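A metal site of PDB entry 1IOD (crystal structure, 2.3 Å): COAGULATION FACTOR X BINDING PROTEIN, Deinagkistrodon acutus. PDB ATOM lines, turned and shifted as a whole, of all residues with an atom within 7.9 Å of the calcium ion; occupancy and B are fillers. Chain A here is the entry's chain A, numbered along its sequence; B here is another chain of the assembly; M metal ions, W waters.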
ATOM      1  N   TYR A   9      19.981  23.238 -27.954  1.00  0.00           N
ATOM      2  CA  TYR A   9      21.099  22.766 -27.158  1.00  0.00           C
ATOM      3  C   TYR A   9      20.642  21.460 -26.549  1.00  0.00           C
ATOM      4  O   TYR A   9      19.669  21.411 -25.800  1.00  0.00           O
ATOM      5  CB  TYR A   9      21.490  23.764 -26.066  1.00  0.00           C
ATOM      6  CG  TYR A   9      22.567  23.219 -25.154  1.00  0.00           C
ATOM      7  CD1 TYR A   9      23.894  23.151 -25.554  1.00  0.00           C
ATOM      8  CD2 TYR A   9      22.229  22.707 -23.907  1.00  0.00           C
ATOM      9  CE1 TYR A   9      24.862  22.584 -24.744  1.00  0.00           C
ATOM     10  CE2 TYR A   9      23.195  22.126 -23.086  1.00  0.00           C
ATOM     11  CZ  TYR A   9      24.498  22.070 -23.513  1.00  0.00           C
ATOM     12  OH  TYR A   9      25.447  21.481 -22.715  1.00  0.00           O
ATOM     13  N   HIS A  12      16.927  20.488 -26.936  1.00  0.00           N
ATOM     14  CA  HIS A  12      16.024  21.313 -26.162  1.00  0.00           C
ATOM     15  C   HIS A  12      16.078  22.669 -26.821  1.00  0.00           C
ATOM     16  O   HIS A  12      17.104  23.038 -27.388  1.00  0.00           O
ATOM     17  CB  HIS A  12      16.466  21.393 -24.702  1.00  0.00           C
ATOM     18  CG  HIS A  12      16.080  20.211 -23.890  1.00  0.00           C
ATOM     19  ND1 HIS A  12      15.102  19.323 -24.285  1.00  0.00           N
ATOM     20  CD2 HIS A  12      16.535  19.757 -22.695  1.00  0.00           C
ATOM     21  CE1 HIS A  12      14.968  18.372 -23.371  1.00  0.00           C
ATOM     22  NE2 HIS A  12      15.822  18.622 -22.397  1.00  0.00           N
ATOM     23  N   TYR A  14      15.431  26.897 -26.483  1.00  0.00           N
ATOM     24  CA  TYR A  14      15.491  27.952 -25.478  1.00  0.00           C
ATOM     25  C   TYR A  14      15.273  29.307 -26.108  1.00  0.00           C
ATOM     26  O   TYR A  14      15.658  29.528 -27.244  1.00  0.00           O
ATOM     27  CB  TYR A  14      16.878  27.993 -24.831  1.00  0.00           C
ATOM     28  CG  TYR A  14      17.390  26.679 -24.277  1.00  0.00           C
ATOM     29  CD1 TYR A  14      17.823  25.666 -25.116  1.00  0.00           C
ATOM     30  CD2 TYR A  14      17.435  26.467 -22.905  1.00  0.00           C
ATOM     31  CE1 TYR A  14      18.296  24.463 -24.604  1.00  0.00           C
ATOM     32  CE2 TYR A  14      17.901  25.284 -22.396  1.00  0.00           C
ATOM     33  CZ  TYR A  14      18.326  24.279 -23.236  1.00  0.00           C
ATOM     34  OH  TYR A  14      18.741  23.087 -22.726  1.00  0.00           O
ATOM     35  N   LEU A  39      10.085  27.551 -17.376  1.00  0.00           N
ATOM     36  CA  LEU A  39      11.237  28.416 -17.171  1.00  0.00           C
ATOM     37  C   LEU A  39      12.427  27.469 -17.323  1.00  0.00           C
ATOM     38  O   LEU A  39      12.305  26.273 -17.050  1.00  0.00           O
ATOM     39  CB  LEU A  39      11.217  29.038 -15.779  1.00  0.00           C
ATOM     40  CG  LEU A  39      10.302  30.254 -15.654  1.00  0.00           C
ATOM     41  CD1 LEU A  39      10.021  30.546 -14.189  1.00  0.00           C
ATOM     42  CD2 LEU A  39      10.943  31.457 -16.335  1.00  0.00           C
ATOM     43  N   VAL A  40      13.544  28.001 -17.796  1.00  0.00           N
ATOM     44  CA  VAL A  40      14.728  27.192 -18.016  1.00  0.00           C
ATOM     45  C   VAL A  40      15.149  26.421 -16.765  1.00  0.00           C
ATOM     46  O   VAL A  40      14.992  26.894 -15.639  1.00  0.00           O
ATOM     47  CB  VAL A  40      15.890  28.071 -18.533  1.00  0.00           C
ATOM     48  CG1 VAL A  40      16.382  29.016 -17.430  1.00  0.00           C
ATOM     49  CG2 VAL A  40      17.002  27.226 -19.081  1.00  0.00           C
ATOM     50  N   SER A  41      15.577  25.172 -16.974  1.00  0.00           N
ATOM     51  CA  SER A  41      16.046  24.325 -15.884  1.00  0.00           C
ATOM     52  C   SER A  41      17.516  24.040 -16.158  1.00  0.00           C
ATOM     53  O   SER A  41      17.845  23.331 -17.119  1.00  0.00           O
ATOM     54  CB  SER A  41      15.245  23.021 -15.842  1.00  0.00           C
ATOM     55  OG  SER A  41      15.236  22.381 -17.116  1.00  0.00           O
ATOM     56  N   ILE A  42      18.386  24.658 -15.377  1.00  0.00           N
ATOM     57  CA  ILE A  42      19.820  24.475 -15.559  1.00  0.00           C
ATOM     58  C   ILE A  42      20.269  23.208 -14.836  1.00  0.00           C
ATOM     59  O   ILE A  42      20.586  23.224 -13.653  1.00  0.00           O
ATOM     60  CB  ILE A  42      20.581  25.714 -15.087  1.00  0.00           C
ATOM     61  CG1 ILE A  42      20.065  26.927 -15.862  1.00  0.00           C
ATOM     62  CG2 ILE A  42      22.067  25.545 -15.320  1.00  0.00           C
ATOM     63  CD1 ILE A  42      20.599  28.237 -15.385  1.00  0.00           C
ATOM     64  N   GLU A  43      20.268  22.116 -15.583  1.00  0.00           N
ATOM     65  CA  GLU A  43      20.631  20.818 -15.039  1.00  0.00           C
ATOM     66  C   GLU A  43      22.063  20.365 -15.233  1.00  0.00           C
ATOM     67  O   GLU A  43      22.396  19.235 -14.904  1.00  0.00           O
ATOM     68  CB  GLU A  43      19.692  19.768 -15.604  1.00  0.00           C
ATOM     69  CG  GLU A  43      18.243  19.979 -15.232  1.00  0.00           C
ATOM     70  CD  GLU A  43      17.334  19.227 -16.158  1.00  0.00           C
ATOM     71  OE1 GLU A  43      17.289  17.984 -16.052  1.00  0.00           O
ATOM     72  OE2 GLU A  43      16.680  19.881 -17.002  1.00  0.00           O
ATOM     73  N   SER A  44      22.919  21.227 -15.768  1.00  0.00           N
ATOM     74  CA  SER A  44      24.297  20.822 -15.954  1.00  0.00           C
ATOM     75  C   SER A  44      25.230  21.986 -16.240  1.00  0.00           C
ATOM     76  O   SER A  44      24.802  23.076 -16.627  1.00  0.00           O
ATOM     77  CB  SER A  44      24.424  19.803 -17.076  1.00  0.00           C
ATOM     78  OG  SER A  44      24.212  20.425 -18.332  1.00  0.00           O
ATOM     79  N   GLU A  47      24.907  23.149 -19.780  1.00  0.00           N
ATOM     80  CA  GLU A  47      23.657  23.865 -20.018  1.00  0.00           C
ATOM     81  C   GLU A  47      23.788  25.273 -19.450  1.00  0.00           C
ATOM     82  O   GLU A  47      23.397  26.241 -20.080  1.00  0.00           O
ATOM     83  CB  GLU A  47      22.479  23.133 -19.377  1.00  0.00           C
ATOM     84  CG  GLU A  47      21.149  23.660 -19.869  1.00  0.00           C
ATOM     85  CD  GLU A  47      19.970  22.903 -19.329  1.00  0.00           C
ATOM     86  OE1 GLU A  47      20.143  21.971 -18.508  1.00  0.00           O
ATOM     87  OE2 GLU A  47      18.839  23.248 -19.735  1.00  0.00           O
ATOM     88  N   VAL A  51      23.239  28.579 -21.661  1.00  0.00           N
ATOM     89  CA  VAL A  51      22.201  29.526 -21.254  1.00  0.00           C
ATOM     90  C   VAL A  51      22.789  30.873 -20.799  1.00  0.00           C
ATOM     91  O   VAL A  51      22.230  31.920 -21.098  1.00  0.00           O
ATOM     92  CB  VAL A  51      21.278  28.919 -20.170  1.00  0.00           C
ATOM     93  CG1 VAL A  51      20.407  29.995 -19.532  1.00  0.00           C
ATOM     94  CG2 VAL A  51      20.374  27.875 -20.800  1.00  0.00           C
ATOM     95  N   GLU A 128      12.332  27.121 -21.774  1.00  0.00           N
ATOM     96  CA  GLU A 128      12.984  25.950 -22.340  1.00  0.00           C
ATOM     97  C   GLU A 128      11.917  24.908 -22.614  1.00  0.00           C
ATOM     98  O   GLU A 128      10.940  24.795 -21.864  1.00  0.00           O
ATOM     99  CB  GLU A 128      14.014  25.370 -21.364  1.00  0.00           C
ATOM    100  CG  GLU A 128      14.636  24.066 -21.860  1.00  0.00           C
ATOM    101  CD  GLU A 128      15.394  23.312 -20.788  1.00  0.00           C
ATOM    102  OE1 GLU A 128      15.769  23.910 -19.757  1.00  0.00           O
ATOM    103  OE2 GLU A 128      15.621  22.107 -20.977  1.00  0.00           O
ATOM    104  N   ALA A 129      12.098  24.161 -23.695  1.00  0.00           N
ATOM    105  CA  ALA A 129      11.185  23.091 -24.091  1.00  0.00           C
ATOM    106  C   ALA A 129      12.054  21.987 -24.709  1.00  0.00           C
ATOM    107  O   ALA A 129      12.341  21.020 -23.987  1.00  0.00           O
ATOM    108  CB  ALA A 129      10.166  23.599 -25.103  1.00  0.00           C
ATOM    109  OXT ALA A 129      12.489  22.124 -25.862  1.00  0.00           O
ATOM    110  N   TRP B  79      12.438  22.290  -9.779  1.00  0.00           N
ATOM    111  CA  TRP B  79      12.285  22.969 -11.056  1.00  0.00           C
ATOM    112  C   TRP B  79      10.811  22.930 -11.435  1.00  0.00           C
ATOM    113  O   TRP B  79      10.087  22.010 -11.055  1.00  0.00           O
ATOM    114  CB  TRP B  79      13.099  22.271 -12.137  1.00  0.00           C
ATOM    115  CG  TRP B  79      14.546  22.311 -11.876  1.00  0.00           C
ATOM    116  CD1 TRP B  79      15.319  21.309 -11.354  1.00  0.00           C
ATOM    117  CD2 TRP B  79      15.415  23.427 -12.082  1.00  0.00           C
ATOM    118  NE1 TRP B  79      16.617  21.736 -11.217  1.00  0.00           N
ATOM    119  CE2 TRP B  79      16.711  23.038 -11.662  1.00  0.00           C
ATOM    120  CE3 TRP B  79      15.233  24.718 -12.590  1.00  0.00           C
ATOM    121  CZ2 TRP B  79      17.811  23.905 -11.711  1.00  0.00           C
ATOM    122  CZ3 TRP B  79      16.329  25.591 -12.651  1.00  0.00           C
ATOM    123  CH2 TRP B  79      17.608  25.174 -12.213  1.00  0.00           C
ATOM    124  N   ASN B  81       9.629  22.277 -14.243  1.00  0.00           N
ATOM    125  CA  ASN B  81       9.408  21.183 -15.186  1.00  0.00           C
ATOM    126  C   ASN B  81       9.589  19.829 -14.512  1.00  0.00           C
ATOM    127  O   ASN B  81       9.677  18.792 -15.172  1.00  0.00           O
ATOM    128  CB  ASN B  81      10.363  21.298 -16.380  1.00  0.00           C
ATOM    129  CG  ASN B  81      11.789  20.961 -16.008  1.00  0.00           C
ATOM    130  OD1 ASN B  81      12.153  20.935 -14.835  1.00  0.00           O
ATOM    131  ND2 ASN B  81      12.608  20.697 -17.021  1.00  0.00           N
ATOM    132  N   ALA B  83      12.174  18.572 -13.249  1.00  0.00           N
ATOM    133  CA  ALA B  83      13.459  17.916 -13.465  1.00  0.00           C
ATOM    134  C   ALA B  83      14.093  17.643 -12.108  1.00  0.00           C
ATOM    135  O   ALA B  83      13.637  18.146 -11.083  1.00  0.00           O
ATOM    136  CB  ALA B  83      14.373  18.780 -14.295  1.00  0.00           C
HETATM  137 CA    CA M   1      17.051  21.833 -18.710  1.00  0.00          CA
HETATM  138  O   HOH W   1      18.356  20.358 -20.086  1.00  0.00           O
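The side-chain hydroxyl of Ser 41 lies close to the side-chain amide nitrogen of Asn 81 of chain B (3.1 Å).
The side-chain hydroxyl (OH) of Tyr 14 lies close to the side-chain carboxylate (OE2) of Glu 47.
N of Glu 47 is in hydrogen-bond range of OG of Ser 44 (3.2 Å).
The side-chain hydroxyl (OH) of Tyr 9 sits at hydrogen-bond distance from the backbone NH (N) of Glu 47.
Four residues have an atom within 4 Å of the calcium ion: Ser 41, Glu 43, Glu 47 and Glu 128.
The calcium ion is bound by O of Ser 41 (2.3 Å), water W1 (2.4 Å), OG of Ser 41 (2.5 Å), OE2 of Glu 47 (2.5 Å), OE2 of Glu 43 (2.6 Å), OE1 of Glu 128 (2.7 Å) and OE2 of Glu 128 (2.7 Å).
The calcium ion has seven donor atoms within binding distance.
Slightly farther from the calcium ion lies OE1 of Glu 47 (3.1 Å).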
